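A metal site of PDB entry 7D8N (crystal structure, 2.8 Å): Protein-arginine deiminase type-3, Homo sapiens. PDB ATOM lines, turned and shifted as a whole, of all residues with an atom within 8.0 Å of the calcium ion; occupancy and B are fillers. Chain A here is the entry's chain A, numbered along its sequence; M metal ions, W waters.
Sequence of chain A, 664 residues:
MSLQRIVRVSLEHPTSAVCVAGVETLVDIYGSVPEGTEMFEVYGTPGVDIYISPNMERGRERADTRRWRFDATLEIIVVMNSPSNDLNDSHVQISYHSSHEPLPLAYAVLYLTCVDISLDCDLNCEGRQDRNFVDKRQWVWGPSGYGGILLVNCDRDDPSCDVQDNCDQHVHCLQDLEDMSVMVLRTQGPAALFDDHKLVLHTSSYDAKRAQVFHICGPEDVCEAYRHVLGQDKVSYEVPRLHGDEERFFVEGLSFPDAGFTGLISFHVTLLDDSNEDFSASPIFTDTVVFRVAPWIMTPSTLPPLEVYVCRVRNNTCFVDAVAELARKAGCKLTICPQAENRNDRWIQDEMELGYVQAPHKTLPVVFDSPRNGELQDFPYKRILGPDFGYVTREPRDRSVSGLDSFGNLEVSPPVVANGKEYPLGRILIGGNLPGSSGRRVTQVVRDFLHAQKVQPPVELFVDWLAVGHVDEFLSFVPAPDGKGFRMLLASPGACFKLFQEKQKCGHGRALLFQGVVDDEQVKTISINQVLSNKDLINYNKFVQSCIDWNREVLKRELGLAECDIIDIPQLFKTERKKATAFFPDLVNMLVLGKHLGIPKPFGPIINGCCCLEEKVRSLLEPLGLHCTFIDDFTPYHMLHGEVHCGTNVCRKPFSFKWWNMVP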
ATOM      1  N   MET A 298     -14.129  22.604 -26.278  1.00  0.00           N
ATOM      2  CA  MET A 298     -14.819  23.667 -25.553  1.00  0.00           C
ATOM      3  C   MET A 298     -15.261  24.775 -26.500  1.00  0.00           C
ATOM      4  O   MET A 298     -14.653  25.014 -27.550  1.00  0.00           O
ATOM      5  CB  MET A 298     -13.911  24.280 -24.477  1.00  0.00           C
ATOM      6  CG  MET A 298     -13.825  23.462 -23.202  1.00  0.00           C
ATOM      7  SD  MET A 298     -12.930  24.309 -21.884  1.00  0.00           S
ATOM      8  CE  MET A 298     -13.982  25.734 -21.607  1.00  0.00           C
ATOM      9  N   ARG A 346     -22.679  28.105  -6.817  1.00  0.00           N
ATOM     10  CA  ARG A 346     -22.706  28.309  -8.263  1.00  0.00           C
ATOM     11  C   ARG A 346     -22.400  26.990  -8.972  1.00  0.00           C
ATOM     12  O   ARG A 346     -21.336  26.800  -9.556  1.00  0.00           O
ATOM     13  CB  ARG A 346     -21.724  29.402  -8.651  1.00  0.00           C
ATOM     14  CG  ARG A 346     -22.064  30.133  -9.941  1.00  0.00           C
ATOM     15  CD  ARG A 346     -20.822  30.418 -10.769  1.00  0.00           C
ATOM     16  NE  ARG A 346     -19.792  31.144 -10.041  1.00  0.00           N
ATOM     17  CZ  ARG A 346     -18.606  31.471 -10.549  1.00  0.00           C
ATOM     18  NH1 ARG A 346     -18.287  31.128 -11.788  1.00  0.00           N
ATOM     19  NH2 ARG A 346     -17.730  32.138  -9.807  1.00  0.00           N
ATOM     20  N   ILE A 348     -24.112  25.780 -11.592  1.00  0.00           N
ATOM     21  CA  ILE A 348     -24.425  25.780 -13.010  1.00  0.00           C
ATOM     22  C   ILE A 348     -23.153  26.033 -13.816  1.00  0.00           C
ATOM     23  O   ILE A 348     -22.979  25.484 -14.901  1.00  0.00           O
ATOM     24  CB  ILE A 348     -25.506  26.828 -13.323  1.00  0.00           C
ATOM     25  CG1 ILE A 348     -26.785  26.530 -12.528  1.00  0.00           C
ATOM     26  CG2 ILE A 348     -25.829  26.848 -14.798  1.00  0.00           C
ATOM     27  CD1 ILE A 348     -27.519  25.309 -13.023  1.00  0.00           C
ATOM     28  N   GLN A 349     -22.248  26.862 -13.280  1.00  0.00           N
ATOM     29  CA  GLN A 349     -21.052  27.298 -13.997  1.00  0.00           C
ATOM     30  C   GLN A 349     -19.784  26.613 -13.517  1.00  0.00           C
ATOM     31  O   GLN A 349     -18.801  26.576 -14.260  1.00  0.00           O
ATOM     32  CB  GLN A 349     -20.895  28.816 -13.868  1.00  0.00           C
ATOM     33  CG  GLN A 349     -19.929  29.442 -14.870  1.00  0.00           C
ATOM     34  CD  GLN A 349     -19.991  30.964 -14.874  1.00  0.00           C
ATOM     35  OE1 GLN A 349     -20.846  31.558 -14.206  1.00  0.00           O
ATOM     36  NE2 GLN A 349     -19.098  31.599 -15.618  1.00  0.00           N
ATOM     37  N   ASP A 350     -19.776  26.080 -12.287  1.00  0.00           N
ATOM     38  CA  ASP A 350     -18.561  25.518 -11.702  1.00  0.00           C
ATOM     39  C   ASP A 350     -18.528  23.996 -11.696  1.00  0.00           C
ATOM     40  O   ASP A 350     -17.435  23.414 -11.712  1.00  0.00           O
ATOM     41  CB  ASP A 350     -18.391  26.018 -10.264  1.00  0.00           C
ATOM     42  CG  ASP A 350     -18.186  27.517 -10.183  1.00  0.00           C
ATOM     43  OD1 ASP A 350     -17.766  28.121 -11.192  1.00  0.00           O
ATOM     44  OD2 ASP A 350     -18.432  28.097  -9.101  1.00  0.00           O
ATOM     45  N   GLU A 351     -19.670  23.334 -11.674  1.00  0.00           N
ATOM     46  CA  GLU A 351     -19.698  21.873 -11.613  1.00  0.00           C
ATOM     47  C   GLU A 351     -19.862  21.218 -12.975  1.00  0.00           C
ATOM     48  O   GLU A 351     -19.943  19.991 -13.047  1.00  0.00           O
ATOM     49  CB  GLU A 351     -20.818  21.403 -10.674  1.00  0.00           C
ATOM     50  CG  GLU A 351     -20.520  21.591  -9.199  1.00  0.00           C
ATOM     51  CD  GLU A 351     -21.488  20.842  -8.300  1.00  0.00           C
ATOM     52  OE1 GLU A 351     -22.518  20.350  -8.804  1.00  0.00           O
ATOM     53  OE2 GLU A 351     -21.220  20.746  -7.081  1.00  0.00           O
ATOM     54  N   MET A 352     -19.873  21.993 -14.057  1.00  0.00           N
ATOM     55  CA  MET A 352     -20.022  21.405 -15.379  1.00  0.00           C
ATOM     56  C   MET A 352     -19.497  22.370 -16.426  1.00  0.00           C
ATOM     57  O   MET A 352     -19.566  23.586 -16.254  1.00  0.00           O
ATOM     58  CB  MET A 352     -21.489  21.034 -15.666  1.00  0.00           C
ATOM     59  CG  MET A 352     -22.428  22.229 -15.768  1.00  0.00           C
ATOM     60  SD  MET A 352     -24.084  21.767 -16.322  1.00  0.00           S
ATOM     61  CE  MET A 352     -24.870  23.369 -16.487  1.00  0.00           C
ATOM     62  N   GLU A 353     -18.975  21.807 -17.505  1.00  0.00           N
ATOM     63  CA  GLU A 353     -18.580  22.556 -18.688  1.00  0.00           C
ATOM     64  C   GLU A 353     -19.289  21.950 -19.890  1.00  0.00           C
ATOM     65  O   GLU A 353     -19.610  20.760 -19.910  1.00  0.00           O
ATOM     66  CB  GLU A 353     -17.061  22.524 -18.897  1.00  0.00           C
ATOM     67  CG  GLU A 353     -16.536  23.666 -19.749  1.00  0.00           C
ATOM     68  CD  GLU A 353     -16.731  25.019 -19.086  1.00  0.00           C
ATOM     69  OE1 GLU A 353     -16.252  25.200 -17.944  1.00  0.00           O
ATOM     70  OE2 GLU A 353     -17.365  25.897 -19.703  1.00  0.00           O
ATOM     71  N   LEU A 354     -19.574  22.783 -20.889  1.00  0.00           N
ATOM     72  CA  LEU A 354     -20.334  22.360 -22.055  1.00  0.00           C
ATOM     73  C   LEU A 354     -19.463  22.456 -23.290  1.00  0.00           C
ATOM     74  O   LEU A 354     -19.033  23.555 -23.663  1.00  0.00           O
ATOM     75  CB  LEU A 354     -21.596  23.214 -22.213  1.00  0.00           C
ATOM     76  CG  LEU A 354     -22.590  23.112 -21.046  1.00  0.00           C
ATOM     77  CD1 LEU A 354     -23.661  24.178 -21.146  1.00  0.00           C
ATOM     78  CD2 LEU A 354     -23.215  21.729 -21.002  1.00  0.00           C
ATOM     79  N   SER A 406     -13.054  22.863  -9.563  1.00  0.00           N
ATOM     80  CA  SER A 406     -14.107  23.822  -9.883  1.00  0.00           C
ATOM     81  C   SER A 406     -13.897  24.292 -11.320  1.00  0.00           C
ATOM     82  O   SER A 406     -12.846  24.848 -11.638  1.00  0.00           O
ATOM     83  CB  SER A 406     -14.106  24.998  -8.916  1.00  0.00           C
ATOM     84  OG  SER A 406     -14.935  26.037  -9.398  1.00  0.00           O
ATOM     85  N   PHE A 407     -14.899  24.089 -12.163  1.00  0.00           N
ATOM     86  CA  PHE A 407     -14.715  24.485 -13.564  1.00  0.00           C
ATOM     87  C   PHE A 407     -14.794  25.993 -13.775  1.00  0.00           C
ATOM     88  O   PHE A 407     -14.839  26.445 -14.927  1.00  0.00           O
ATOM     89  CB  PHE A 407     -15.725  23.766 -14.455  1.00  0.00           C
ATOM     90  CG  PHE A 407     -15.361  22.333 -14.744  1.00  0.00           C
ATOM     91  CD1 PHE A 407     -14.109  21.839 -14.392  1.00  0.00           C
ATOM     92  CD2 PHE A 407     -16.269  21.479 -15.350  1.00  0.00           C
ATOM     93  CE1 PHE A 407     -13.774  20.520 -14.658  1.00  0.00           C
ATOM     94  CE2 PHE A 407     -15.941  20.164 -15.609  1.00  0.00           C
ATOM     95  CZ  PHE A 407     -14.682  19.683 -15.258  1.00  0.00           C
ATOM     96  N   GLY A 408     -14.831  26.789 -12.699  1.00  0.00           N
ATOM     97  CA  GLY A 408     -14.550  28.197 -12.818  1.00  0.00           C
ATOM     98  C   GLY A 408     -13.089  28.503 -13.085  1.00  0.00           C
ATOM     99  O   GLY A 408     -12.768  29.628 -13.498  1.00  0.00           O
ATOM    100  N   ASN A 409     -12.203  27.536 -12.832  1.00  0.00           N
ATOM    101  CA  ASN A 409     -10.801  27.619 -13.233  1.00  0.00           C
ATOM    102  C   ASN A 409     -10.585  27.261 -14.692  1.00  0.00           C
ATOM    103  O   ASN A 409      -9.439  27.232 -15.143  1.00  0.00           O
ATOM    104  CB  ASN A 409      -9.948  26.686 -12.366  1.00  0.00           C
ATOM    105  CG  ASN A 409     -10.104  26.964 -10.887  1.00  0.00           C
ATOM    106  OD1 ASN A 409     -10.016  28.104 -10.439  1.00  0.00           O
ATOM    107  ND2 ASN A 409     -10.344  25.904 -10.114  1.00  0.00           N
ATOM    108  N   LEU A 410     -11.659  26.979 -15.433  1.00  0.00           N
ATOM    109  CA  LEU A 410     -11.578  26.479 -16.803  1.00  0.00           C
ATOM    110  C   LEU A 410     -12.321  27.431 -17.722  1.00  0.00           C
ATOM    111  O   LEU A 410     -13.519  27.664 -17.531  1.00  0.00           O
ATOM    112  CB  LEU A 410     -12.167  25.072 -16.900  1.00  0.00           C
ATOM    113  CG  LEU A 410     -11.379  24.079 -17.740  1.00  0.00           C
ATOM    114  CD1 LEU A 410      -9.999  23.895 -17.138  1.00  0.00           C
ATOM    115  CD2 LEU A 410     -12.111  22.750 -17.837  1.00  0.00           C
ATOM    116  N   GLU A 411     -11.615  27.975 -18.716  1.00  0.00           N
ATOM    117  CA  GLU A 411     -12.249  28.764 -19.766  1.00  0.00           C
ATOM    118  C   GLU A 411     -11.552  28.443 -21.088  1.00  0.00           C
ATOM    119  O   GLU A 411     -10.669  27.589 -21.142  1.00  0.00           O
ATOM    120  CB  GLU A 411     -12.188  30.270 -19.459  1.00  0.00           C
ATOM    121  CG  GLU A 411     -13.050  30.725 -18.280  1.00  0.00           C
ATOM    122  CD  GLU A 411     -14.518  30.367 -18.446  1.00  0.00           C
ATOM    123  OE1 GLU A 411     -15.169  29.996 -17.439  1.00  0.00           O
ATOM    124  OE2 GLU A 411     -15.038  30.468 -19.588  1.00  0.00           O
ATOM    125  N   VAL A 412     -11.937  29.134 -22.156  1.00  0.00           N
ATOM    126  CA  VAL A 412     -11.334  28.914 -23.467  1.00  0.00           C
ATOM    127  C   VAL A 412     -11.432  30.209 -24.266  1.00  0.00           C
ATOM    128  O   VAL A 412     -12.358  30.994 -24.099  1.00  0.00           O
ATOM    129  CB  VAL A 412     -12.002  27.721 -24.204  1.00  0.00           C
ATOM    130  CG1 VAL A 412     -13.448  28.032 -24.556  1.00  0.00           C
ATOM    131  CG2 VAL A 412     -11.208  27.341 -25.443  1.00  0.00           C
ATOM    132  N   LEU A 429      -7.838  27.838 -21.212  1.00  0.00           N
ATOM    133  CA  LEU A 429      -7.176  28.634 -20.189  1.00  0.00           C
ATOM    134  C   LEU A 429      -7.494  28.026 -18.832  1.00  0.00           C
ATOM    135  O   LEU A 429      -8.670  27.931 -18.448  1.00  0.00           O
ATOM    136  CB  LEU A 429      -7.630  30.095 -20.248  1.00  0.00           C
ATOM    137  CG  LEU A 429      -7.591  30.734 -21.643  1.00  0.00           C
ATOM    138  CD1 LEU A 429      -8.308  32.085 -21.647  1.00  0.00           C
ATOM    139  CD2 LEU A 429      -6.167  30.890 -22.132  1.00  0.00           C
ATOM    140  N   VAL A 471     -10.976  31.908 -13.134  1.00  0.00           N
ATOM    141  CA  VAL A 471     -10.487  32.713 -14.247  1.00  0.00           C
ATOM    142  C   VAL A 471     -11.428  33.870 -14.539  1.00  0.00           C
ATOM    143  O   VAL A 471     -11.000  34.998 -14.785  1.00  0.00           O
ATOM    144  CB  VAL A 471     -10.272  31.821 -15.487  1.00  0.00           C
ATOM    145  CG1 VAL A 471     -10.038  32.673 -16.721  1.00  0.00           C
ATOM    146  CG2 VAL A 471      -9.112  30.871 -15.266  1.00  0.00           C
ATOM    147  N   ASP A 472     -12.744  33.614 -14.471  1.00  0.00           N
ATOM    148  CA  ASP A 472     -13.720  34.652 -14.789  1.00  0.00           C
ATOM    149  C   ASP A 472     -13.792  35.758 -13.743  1.00  0.00           C
ATOM    150  O   ASP A 472     -14.629  36.652 -13.876  1.00  0.00           O
ATOM    151  CB  ASP A 472     -15.108  34.030 -15.003  1.00  0.00           C
ATOM    152  CG  ASP A 472     -15.537  33.145 -13.852  1.00  0.00           C
ATOM    153  OD1 ASP A 472     -15.839  33.675 -12.766  1.00  0.00           O
ATOM    154  OD2 ASP A 472     -15.575  31.906 -14.047  1.00  0.00           O
ATOM    155  N   THR A 648     -24.895  30.345 -14.032  1.00  0.00           N
ATOM    156  CA  THR A 648     -25.307  30.458 -15.423  1.00  0.00           C
ATOM    157  C   THR A 648     -24.339  29.664 -16.291  1.00  0.00           C
ATOM    158  O   THR A 648     -23.130  29.658 -16.046  1.00  0.00           O
ATOM    159  CB  THR A 648     -25.369  31.915 -15.877  1.00  0.00           C
ATOM    160  OG1 THR A 648     -25.710  31.972 -17.265  1.00  0.00           O
ATOM    161  CG2 THR A 648     -24.025  32.610 -15.662  1.00  0.00           C
ATOM    162  N   ASN A 649     -24.887  28.960 -17.281  1.00  0.00           N
ATOM    163  CA  ASN A 649     -24.073  28.224 -18.246  1.00  0.00           C
ATOM    164  C   ASN A 649     -24.772  28.254 -19.593  1.00  0.00           C
ATOM    165  O   ASN A 649     -26.003  28.350 -19.676  1.00  0.00           O
ATOM    166  CB  ASN A 649     -23.841  26.778 -17.789  1.00  0.00           C
ATOM    167  CG  ASN A 649     -22.438  26.298 -18.081  1.00  0.00           C
ATOM    168  OD1 ASN A 649     -21.829  26.693 -19.069  1.00  0.00           O
ATOM    169  ND2 ASN A 649     -21.912  25.457 -17.198  1.00  0.00           N
HETATM  170 CA    CA M   1     -16.141  27.565 -17.045  1.00  0.00          CA
HETATM  171  O   HOH W   1     -17.461  29.163 -18.513  1.00  0.00           O
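Gln 349 touches the calcium ion (O to CA, 3.98 Å).
Water W1 bridges the side-chain carboxylate of Glu 411 (3.0 Å) and the side-chain carboxylate of Glu 353 (3.5 Å).
The backbone carbonyl oxygen (O) of Thr 648 lies close to the side-chain amide oxygen (OE1) of Gln 349. O of Glu 411 lies within hydrogen-bond range of N of Leu 429. The backbone carbonyl oxygen (O) of Asp 350 lies within hydrogen-bond range of the backbone NH (N) of Phe 407 (2.7 Å).
The calcium ion is bound by the side-chain carboxylate (OE1) of Glu 353, 2.5 Å away. The calcium ion is bound by water W1, 2.5 Å away. OE1 of Glu 411 binds the calcium ion (2.6 Å). The backbone carbonyl oxygen (O) of Leu 410 is bound to the calcium ion (2.7 Å). O of Phe 407 binds the calcium ion, at 2.7 Å. The calcium ion has five donor atoms within binding distance.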
